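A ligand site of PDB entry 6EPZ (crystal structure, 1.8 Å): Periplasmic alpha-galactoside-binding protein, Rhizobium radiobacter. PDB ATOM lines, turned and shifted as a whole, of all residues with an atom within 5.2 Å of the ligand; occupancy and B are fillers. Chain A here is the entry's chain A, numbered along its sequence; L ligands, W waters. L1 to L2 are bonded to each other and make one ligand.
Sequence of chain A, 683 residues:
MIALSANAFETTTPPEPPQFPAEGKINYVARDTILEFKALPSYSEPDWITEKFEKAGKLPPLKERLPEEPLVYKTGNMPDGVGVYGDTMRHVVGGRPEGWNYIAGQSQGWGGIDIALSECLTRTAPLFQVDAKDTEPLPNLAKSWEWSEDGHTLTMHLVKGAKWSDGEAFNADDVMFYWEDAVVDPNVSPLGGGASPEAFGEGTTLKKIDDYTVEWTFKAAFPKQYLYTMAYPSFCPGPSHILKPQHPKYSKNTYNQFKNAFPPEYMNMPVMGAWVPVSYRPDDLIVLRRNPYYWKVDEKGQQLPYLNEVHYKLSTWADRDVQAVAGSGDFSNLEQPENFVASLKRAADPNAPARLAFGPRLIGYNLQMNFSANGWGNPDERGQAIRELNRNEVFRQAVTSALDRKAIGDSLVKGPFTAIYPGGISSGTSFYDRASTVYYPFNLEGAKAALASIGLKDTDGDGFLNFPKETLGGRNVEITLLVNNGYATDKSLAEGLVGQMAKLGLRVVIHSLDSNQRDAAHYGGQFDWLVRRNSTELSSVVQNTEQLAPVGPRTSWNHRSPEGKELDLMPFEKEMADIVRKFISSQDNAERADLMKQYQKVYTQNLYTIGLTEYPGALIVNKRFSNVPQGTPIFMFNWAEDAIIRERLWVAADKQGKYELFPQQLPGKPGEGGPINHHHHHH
OE2 of Glu 641 lies within hydrogen-bond range of O3 of LG2 L2 (2.5 Å).
The side-chain carboxylate of Glu 335 lies within hydrogen-bond range of an oxygen (O2) of LG2 L2.
The side-chain hydroxyl (OH) of Tyr 487 is in hydrogen-bond range of an oxygen (O1) of LG2 L2, 2.8 Å away.
NH1 of Arg 320 sits at hydrogen-bond distance from O3 of LG2 L2 (2.8 Å).
O1 of LG2 L2 is in hydrogen-bond range of NH2 of Arg 533 (2.9 Å).
The backbone NH of Gly 111 is in hydrogen-bond range of an oxygen (O4) of LG2 L2.
ND2 of Asn 333 lies within hydrogen-bond range of O2 of LG2 L2 (3.1 Å).
An oxygen (O1) of LIG L1 is in hydrogen-bond range of the indole nitrogen (NE1) of Trp 639 (3.1 Å).
Water W4 lies within hydrogen-bond range of the side-chain hydroxyl of Tyr 523 (2.7 Å), an oxygen (O3) of LIG L1 (2.7 Å) and the side-chain carboxylate of Asp 519 (2.7 Å).
Water W2 bridges an oxygen (O5) of LG2 L2 and the side-chain hydroxyl of Tyr 232.
Water W5 lies within hydrogen-bond range of the side-chain carboxylate of Asp 114 (2.6 Å), an oxygen (O5) of LG2 L2 (2.8 Å), the backbone NH of Gly 112 (2.9 Å) and the backbone NH of Ile 115 (3.4 Å).
Water W3 lies within hydrogen-bond range of the backbone carbonyl oxygen of Gly 192 and an oxygen (O2) of LIG L1.
The guanidinium group of Arg 320 is in salt-bridge range of the side-chain carboxylate of Glu 641 (3.5 Å).
OE1 of Glu 641 sits at hydrogen-bond distance from ND2 of Asn 333 (2.9 Å).
The guanidinium group of Arg 320 is in salt-bridge range of the side-chain carboxylate of Glu 335, 3.2 Å away.
NH1 of Arg 533 is in salt-bridge range of OE2 of Glu 335, at 3.1 Å.
NE1 of Trp 317 lies within hydrogen-bond range of OH of Tyr 487, 3.3 Å away.
The backbone carbonyl oxygen of Asn 333 is in hydrogen-bond range of the guanidinium group of Arg 320.
CB of Trp 110 touches O4 of LG2 L2 (3.4 Å).
N of Gly 112 touches C6 of LG2 L2 (3.7 Å).
Ile 115 touches the ligand.
Trp 317 touches the ligand.
12 residues have an atom within 4 Å of the ligand: Trp 110, Gly 111, Gly 112, Ile 115, Trp 317, Arg 320, Asn 333, Glu 335, Tyr 487, Arg 533, Trp 639 and Glu 641.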
ATOM      1  N   TRP A 110      27.528 -17.370  11.315  1.00  0.00           N
ATOM      2  CA  TRP A 110      26.126 -17.635  10.908  1.00  0.00           C
ATOM      3  C   TRP A 110      26.066 -18.341   9.539  1.00  0.00           C
ATOM      4  O   TRP A 110      27.022 -19.028   9.144  1.00  0.00           O
ATOM      5  CB  TRP A 110      25.297 -16.314  10.947  1.00  0.00           C
ATOM      6  CG  TRP A 110      25.351 -15.608  12.262  1.00  0.00           C
ATOM      7  CD1 TRP A 110      25.971 -14.414  12.537  1.00  0.00           C
ATOM      8  CD2 TRP A 110      24.739 -16.033  13.501  1.00  0.00           C
ATOM      9  NE1 TRP A 110      25.783 -14.075  13.858  1.00  0.00           N
ATOM     10  CE2 TRP A 110      24.998 -15.034  14.467  1.00  0.00           C
ATOM     11  CE3 TRP A 110      23.922 -17.134  13.864  1.00  0.00           C
ATOM     12  CZ2 TRP A 110      24.527 -15.122  15.779  1.00  0.00           C
ATOM     13  CZ3 TRP A 110      23.483 -17.231  15.180  1.00  0.00           C
ATOM     14  CH2 TRP A 110      23.762 -16.220  16.116  1.00  0.00           C
ATOM     15  N   GLY A 111      24.951 -18.206   8.823  1.00  0.00           N
ATOM     16  CA  GLY A 111      24.809 -18.805   7.498  1.00  0.00           C
ATOM     17  C   GLY A 111      24.979 -20.311   7.445  1.00  0.00           C
ATOM     18  O   GLY A 111      25.318 -20.856   6.402  1.00  0.00           O
ATOM     19  N   GLY A 112      24.764 -20.989   8.583  1.00  0.00           N
ATOM     20  CA  GLY A 112      24.775 -22.452   8.656  1.00  0.00           C
ATOM     21  C   GLY A 112      25.951 -23.070   9.379  1.00  0.00           C
ATOM     22  O   GLY A 112      25.918 -24.273   9.673  1.00  0.00           O
ATOM     23  N   ASP A 114      27.378 -22.538  12.611  1.00  0.00           N
ATOM     24  CA  ASP A 114      27.124 -23.038  13.969  1.00  0.00           C
ATOM     25  C   ASP A 114      25.969 -24.049  13.977  1.00  0.00           C
ATOM     26  O   ASP A 114      25.984 -24.974  14.778  1.00  0.00           O
ATOM     27  CB  ASP A 114      26.880 -21.911  14.960  1.00  0.00           C
ATOM     28  CG  ASP A 114      25.724 -21.028  14.539  1.00  0.00           C
ATOM     29  OD1 ASP A 114      25.874 -20.296  13.528  1.00  0.00           O
ATOM     30  OD2 ASP A 114      24.674 -21.082  15.215  1.00  0.00           O
ATOM     31  N   ILE A 115      25.024 -23.928  13.010  1.00  0.00           N
ATOM     32  CA  ILE A 115      23.929 -24.897  12.915  1.00  0.00           C
ATOM     33  C   ILE A 115      24.502 -26.304  12.667  1.00  0.00           C
ATOM     34  O   ILE A 115      24.063 -27.242  13.332  1.00  0.00           O
ATOM     35  CB  ILE A 115      22.920 -24.467  11.822  1.00  0.00           C
ATOM     36  CG1 ILE A 115      22.067 -23.267  12.339  1.00  0.00           C
ATOM     37  CG2 ILE A 115      22.019 -25.671  11.379  1.00  0.00           C
ATOM     38  CD1 ILE A 115      21.230 -22.562  11.255  1.00  0.00           C
ATOM     39  N   GLY A 192      23.183 -16.274  20.703  1.00  0.00           N
ATOM     40  CA  GLY A 192      21.799 -16.065  20.315  1.00  0.00           C
ATOM     41  C   GLY A 192      20.941 -15.172  21.188  1.00  0.00           C
ATOM     42  O   GLY A 192      19.854 -14.767  20.772  1.00  0.00           O
ATOM     43  N   TYR A 232      17.995 -26.252  18.728  1.00  0.00           N
ATOM     44  CA  TYR A 232      18.814 -25.080  18.368  1.00  0.00           C
ATOM     45  C   TYR A 232      17.962 -23.800  18.547  1.00  0.00           C
ATOM     46  O   TYR A 232      16.797 -23.801  18.136  1.00  0.00           O
ATOM     47  CB  TYR A 232      19.309 -25.194  16.918  1.00  0.00           C
ATOM     48  CG  TYR A 232      20.091 -23.980  16.461  1.00  0.00           C
ATOM     49  CD1 TYR A 232      19.437 -22.878  15.924  1.00  0.00           C
ATOM     50  CD2 TYR A 232      21.483 -23.959  16.531  1.00  0.00           C
ATOM     51  CE1 TYR A 232      20.140 -21.761  15.485  1.00  0.00           C
ATOM     52  CE2 TYR A 232      22.205 -22.839  16.082  1.00  0.00           C
ATOM     53  CZ  TYR A 232      21.524 -21.745  15.558  1.00  0.00           C
ATOM     54  OH  TYR A 232      22.159 -20.627  15.074  1.00  0.00           O
ATOM     55  N   TRP A 317      26.151 -10.918   2.815  1.00  0.00           N
ATOM     56  CA  TRP A 317      24.867 -11.610   2.709  1.00  0.00           C
ATOM     57  C   TRP A 317      24.278 -11.444   1.282  1.00  0.00           C
ATOM     58  O   TRP A 317      23.766 -12.419   0.738  1.00  0.00           O
ATOM     59  CB  TRP A 317      23.871 -11.191   3.820  1.00  0.00           C
ATOM     60  CG  TRP A 317      24.363 -11.583   5.188  1.00  0.00           C
ATOM     61  CD1 TRP A 317      24.762 -10.737   6.185  1.00  0.00           C
ATOM     62  CD2 TRP A 317      24.618 -12.912   5.660  1.00  0.00           C
ATOM     63  NE1 TRP A 317      25.191 -11.465   7.279  1.00  0.00           N
ATOM     64  CE2 TRP A 317      25.099 -12.803   6.986  1.00  0.00           C
ATOM     65  CE3 TRP A 317      24.397 -14.207   5.122  1.00  0.00           C
ATOM     66  CZ2 TRP A 317      25.428 -13.927   7.765  1.00  0.00           C
ATOM     67  CZ3 TRP A 317      24.769 -15.319   5.870  1.00  0.00           C
ATOM     68  CH2 TRP A 317      25.250 -15.179   7.181  1.00  0.00           C
ATOM     69  N   ARG A 320      25.794 -13.887  -1.224  1.00  0.00           N
ATOM     70  CA  ARG A 320      25.291 -15.278  -1.122  1.00  0.00           C
ATOM     71  C   ARG A 320      24.237 -15.523  -2.197  1.00  0.00           C
ATOM     72  O   ARG A 320      24.293 -16.564  -2.853  1.00  0.00           O
ATOM     73  CB  ARG A 320      24.752 -15.581   0.267  1.00  0.00           C
ATOM     74  CG  ARG A 320      24.246 -17.032   0.391  1.00  0.00           C
ATOM     75  CD  ARG A 320      23.696 -17.382   1.764  1.00  0.00           C
ATOM     76  NE  ARG A 320      22.553 -16.552   2.150  1.00  0.00           N
ATOM     77  CZ  ARG A 320      21.982 -16.594   3.340  1.00  0.00           C
ATOM     78  NH1 ARG A 320      22.426 -17.432   4.275  1.00  0.00           N
ATOM     79  NH2 ARG A 320      20.979 -15.782   3.628  1.00  0.00           N
ATOM     80  N   ASN A 333      19.417 -18.288   1.278  1.00  0.00           N
ATOM     81  CA  ASN A 333      18.106 -17.883   1.768  1.00  0.00           C
ATOM     82  C   ASN A 333      17.915 -16.483   1.187  1.00  0.00           C
ATOM     83  O   ASN A 333      18.575 -15.526   1.617  1.00  0.00           O
ATOM     84  CB  ASN A 333      18.034 -17.867   3.300  1.00  0.00           C
ATOM     85  CG  ASN A 333      18.225 -19.227   3.924  1.00  0.00           C
ATOM     86  OD1 ASN A 333      17.698 -20.237   3.413  1.00  0.00           O
ATOM     87  ND2 ASN A 333      18.970 -19.300   5.016  1.00  0.00           N
ATOM     88  N   GLU A 335      16.271 -13.515   1.183  1.00  0.00           N
ATOM     89  CA  GLU A 335      15.480 -12.909   2.267  1.00  0.00           C
ATOM     90  C   GLU A 335      15.521 -11.389   2.306  1.00  0.00           C
ATOM     91  O   GLU A 335      14.969 -10.794   3.230  1.00  0.00           O
ATOM     92  CB  GLU A 335      16.034 -13.470   3.598  1.00  0.00           C
ATOM     93  CG  GLU A 335      17.491 -13.073   3.812  1.00  0.00           C
ATOM     94  CD  GLU A 335      18.270 -13.846   4.853  1.00  0.00           C
ATOM     95  OE1 GLU A 335      17.711 -14.782   5.466  1.00  0.00           O
ATOM     96  OE2 GLU A 335      19.419 -13.445   5.123  1.00  0.00           O
ATOM     97  N   ASN A 484      21.479  -3.552  12.493  1.00  0.00           N
ATOM     98  CA  ASN A 484      22.482  -4.528  12.042  1.00  0.00           C
ATOM     99  C   ASN A 484      23.014  -4.011  10.682  1.00  0.00           C
ATOM    100  O   ASN A 484      22.274  -3.969   9.684  1.00  0.00           O
ATOM    101  CB  ASN A 484      21.820  -5.919  11.881  1.00  0.00           C
ATOM    102  CG  ASN A 484      22.823  -7.016  11.655  1.00  0.00           C
ATOM    103  OD1 ASN A 484      23.816  -6.845  10.931  1.00  0.00           O
ATOM    104  ND2 ASN A 484      22.606  -8.162  12.274  1.00  0.00           N
ATOM    105  N   TYR A 487      22.994  -5.988   6.594  1.00  0.00           N
ATOM    106  CA  TYR A 487      21.893  -6.216   5.662  1.00  0.00           C
ATOM    107  C   TYR A 487      21.357  -4.944   5.069  1.00  0.00           C
ATOM    108  O   TYR A 487      21.053  -3.993   5.809  1.00  0.00           O
ATOM    109  CB  TYR A 487      20.743  -6.976   6.389  1.00  0.00           C
ATOM    110  CG  TYR A 487      21.128  -8.336   6.959  1.00  0.00           C
ATOM    111  CD1 TYR A 487      21.681  -8.435   8.236  1.00  0.00           C
ATOM    112  CD2 TYR A 487      20.926  -9.496   6.236  1.00  0.00           C
ATOM    113  CE1 TYR A 487      22.058  -9.678   8.756  1.00  0.00           C
ATOM    114  CE2 TYR A 487      21.251 -10.753   6.758  1.00  0.00           C
ATOM    115  CZ  TYR A 487      21.839 -10.824   8.011  1.00  0.00           C
ATOM    116  OH  TYR A 487      22.179 -12.049   8.532  1.00  0.00           O
ATOM    117  N   SER A 515      27.184  -7.243  13.367  1.00  0.00           N
ATOM    118  CA  SER A 515      26.380  -8.243  14.090  1.00  0.00           C
ATOM    119  C   SER A 515      26.779  -8.461  15.557  1.00  0.00           C
ATOM    120  O   SER A 515      25.911  -8.399  16.430  1.00  0.00           O
ATOM    121  CB  SER A 515      26.347  -9.567  13.324  1.00  0.00           C
ATOM    122  OG  SER A 515      25.486 -10.507  13.965  1.00  0.00           O
ATOM    123  N   ASP A 519      24.632  -7.253  18.793  1.00  0.00           N
ATOM    124  CA  ASP A 519      24.149  -8.234  19.781  1.00  0.00           C
ATOM    125  C   ASP A 519      24.519  -7.813  21.201  1.00  0.00           C
ATOM    126  O   ASP A 519      23.653  -7.841  22.087  1.00  0.00           O
ATOM    127  CB  ASP A 519      24.724  -9.616  19.480  1.00  0.00           C
ATOM    128  CG  ASP A 519      24.040 -10.338  18.336  1.00  0.00           C
ATOM    129  OD1 ASP A 519      23.059  -9.774  17.776  1.00  0.00           O
ATOM    130  OD2 ASP A 519      24.493 -11.458  17.974  1.00  0.00           O
ATOM    131  N   TYR A 523      21.469  -7.188  23.817  1.00  0.00           N
ATOM    132  CA  TYR A 523      21.340  -8.056  24.981  1.00  0.00           C
ATOM    133  C   TYR A 523      21.806  -7.364  26.265  1.00  0.00           C
ATOM    134  O   TYR A 523      21.240  -7.602  27.316  1.00  0.00           O
ATOM    135  CB  TYR A 523      21.987  -9.456  24.742  1.00  0.00           C
ATOM    136  CG  TYR A 523      21.579 -10.073  23.412  1.00  0.00           C
ATOM    137  CD1 TYR A 523      20.330  -9.823  22.849  1.00  0.00           C
ATOM    138  CD2 TYR A 523      22.459 -10.890  22.705  1.00  0.00           C
ATOM    139  CE1 TYR A 523      19.985 -10.324  21.593  1.00  0.00           C
ATOM    140  CE2 TYR A 523      22.115 -11.422  21.464  1.00  0.00           C
ATOM    141  CZ  TYR A 523      20.874 -11.138  20.916  1.00  0.00           C
ATOM    142  OH  TYR A 523      20.513 -11.637  19.691  1.00  0.00           O
ATOM    143  N   ARG A 533      14.930  -8.307  12.478  1.00  0.00           N
ATOM    144  CA  ARG A 533      14.223  -9.352  11.754  1.00  0.00           C
ATOM    145  C   ARG A 533      13.691 -10.347  12.821  1.00  0.00           C
ATOM    146  O   ARG A 533      14.399 -10.651  13.799  1.00  0.00           O
ATOM    147  CB  ARG A 533      15.188 -10.030  10.771  1.00  0.00           C
ATOM    148  CG  ARG A 533      14.466 -11.008   9.817  1.00  0.00           C
ATOM    149  CD  ARG A 533      15.395 -11.514   8.743  1.00  0.00           C
ATOM    150  NE  ARG A 533      16.558 -12.175   9.314  1.00  0.00           N
ATOM    151  CZ  ARG A 533      17.679 -12.430   8.646  1.00  0.00           C
ATOM    152  NH1 ARG A 533      17.784 -12.077   7.365  1.00  0.00           N
ATOM    153  NH2 ARG A 533      18.678 -13.067   9.226  1.00  0.00           N
ATOM    154  N   PHE A 635      12.724 -20.055   6.664  1.00  0.00           N
ATOM    155  CA  PHE A 635      12.723 -19.837   8.102  1.00  0.00           C
ATOM    156  C   PHE A 635      11.347 -20.155   8.713  1.00  0.00           C
ATOM    157  O   PHE A 635      10.356 -19.570   8.300  1.00  0.00           O
ATOM    158  CB  PHE A 635      13.101 -18.353   8.384  1.00  0.00           C
ATOM    159  CG  PHE A 635      13.237 -17.992   9.842  1.00  0.00           C
ATOM    160  CD1 PHE A 635      14.325 -18.431  10.582  1.00  0.00           C
ATOM    161  CD2 PHE A 635      12.300 -17.175  10.464  1.00  0.00           C
ATOM    162  CE1 PHE A 635      14.476 -18.059  11.932  1.00  0.00           C
ATOM    163  CE2 PHE A 635      12.432 -16.827  11.818  1.00  0.00           C
ATOM    164  CZ  PHE A 635      13.547 -17.249  12.525  1.00  0.00           C
ATOM    165  N   TRP A 639      16.294 -21.910  10.441  1.00  0.00           N
ATOM    166  CA  TRP A 639      16.703 -21.586   9.077  1.00  0.00           C
ATOM    167  C   TRP A 639      16.735 -22.863   8.230  1.00  0.00           C
ATOM    168  O   TRP A 639      16.927 -23.966   8.775  1.00  0.00           O
ATOM    169  CB  TRP A 639      18.090 -20.909   9.093  1.00  0.00           C
ATOM    170  CG  TRP A 639      18.052 -19.547   9.733  1.00  0.00           C
ATOM    171  CD1 TRP A 639      18.414 -19.230  11.007  1.00  0.00           C
ATOM    172  CD2 TRP A 639      17.490 -18.373   9.165  1.00  0.00           C
ATOM    173  NE1 TRP A 639      18.084 -17.909  11.283  1.00  0.00           N
ATOM    174  CE2 TRP A 639      17.542 -17.353  10.151  1.00  0.00           C
ATOM    175  CE3 TRP A 639      16.938 -18.061   7.902  1.00  0.00           C
ATOM    176  CZ2 TRP A 639      17.069 -16.054   9.922  1.00  0.00           C
ATOM    177  CZ3 TRP A 639      16.434 -16.778   7.697  1.00  0.00           C
ATOM    178  CH2 TRP A 639      16.503 -15.800   8.687  1.00  0.00           C
ATOM    179  N   GLU A 641      19.038 -24.038   6.423  1.00  0.00           N
ATOM    180  CA  GLU A 641      20.312 -24.787   6.585  1.00  0.00           C
ATOM    181  C   GLU A 641      20.109 -25.991   7.515  1.00  0.00           C
ATOM    182  O   GLU A 641      20.689 -27.053   7.262  1.00  0.00           O
ATOM    183  CB  GLU A 641      21.455 -23.897   7.118  1.00  0.00           C
ATOM    184  CG  GLU A 641      21.973 -22.881   6.120  1.00  0.00           C
ATOM    185  CD  GLU A 641      21.332 -21.506   6.190  1.00  0.00           C
ATOM    186  OE1 GLU A 641      20.153 -21.406   6.589  1.00  0.00           O
ATOM    187  OE2 GLU A 641      22.023 -20.524   5.818  1.00  0.00           O
HETATM  188  C1  LIG L   1      20.011 -16.054  13.894  1.00  0.00           C
HETATM  189  C2  LIG L   1      20.333 -15.046  15.083  1.00  0.00           C
HETATM  190  C3  LIG L   1      20.657 -13.604  14.614  1.00  0.00           C
HETATM  191  C4  LIG L   1      21.545 -13.625  13.350  1.00  0.00           C
HETATM  192  C5  LIG L   1      20.817 -14.281  12.175  1.00  0.00           C
HETATM  193  C6  LIG L   1      21.850 -14.625  11.096  1.00  0.00           C
HETATM  194  O1  LIG L   1      18.806 -16.808  14.100  1.00  0.00           O
HETATM  195  O2  LIG L   1      19.303 -15.008  16.091  1.00  0.00           O
HETATM  196  O3  LIG L   1      21.405 -12.982  15.679  1.00  0.00           O
HETATM  197  O4  LIG L   1      21.899 -12.294  12.967  1.00  0.00           O
HETATM  198  O5  LIG L   1      19.961 -15.430  12.548  1.00  0.00           O
HETATM  199  O6  LIG L   1      21.140 -14.922   9.901  1.00  0.00           O
HETATM  200  C1  LG2 L   2      21.996 -15.411   8.868  1.00  0.00           C
HETATM  201  C2  LG2 L   2      21.271 -15.326   7.470  1.00  0.00           C
HETATM  202  C3  LG2 L   2      20.143 -16.392   7.417  1.00  0.00           C
HETATM  203  C4  LG2 L   2      20.608 -17.769   7.827  1.00  0.00           C
HETATM  204  C5  LG2 L   2      21.302 -17.718   9.215  1.00  0.00           C
HETATM  205  C6  LG2 L   2      21.783 -19.113   9.602  1.00  0.00           C
HETATM  206  O1  LG2 L   2      20.669 -14.036   7.352  1.00  0.00           O
HETATM  207  O2  LG2 L   2      19.592 -16.488   6.095  1.00  0.00           O
HETATM  208  O3  LG2 L   2      21.544 -18.246   6.825  1.00  0.00           O
HETATM  209  O4  LG2 L   2      22.410 -16.769   9.137  1.00  0.00           O
HETATM  210  O5  LG2 L   2      22.431 -19.070  10.884  1.00  0.00           O
HETATM  211  O   HOH W   1      20.294 -17.853  17.364  1.00  0.00           O
HETATM  212  O   HOH W   2      20.939 -19.054  13.180  1.00  0.00           O
HETATM  213  O   HOH W   3      18.395 -16.546  18.833  1.00  0.00           O
HETATM  214  O   HOH W   4      22.284 -13.042  18.243  1.00  0.00           O
HETATM  215  O   HOH W   5      24.443 -20.941  11.432  1.00  0.00           O
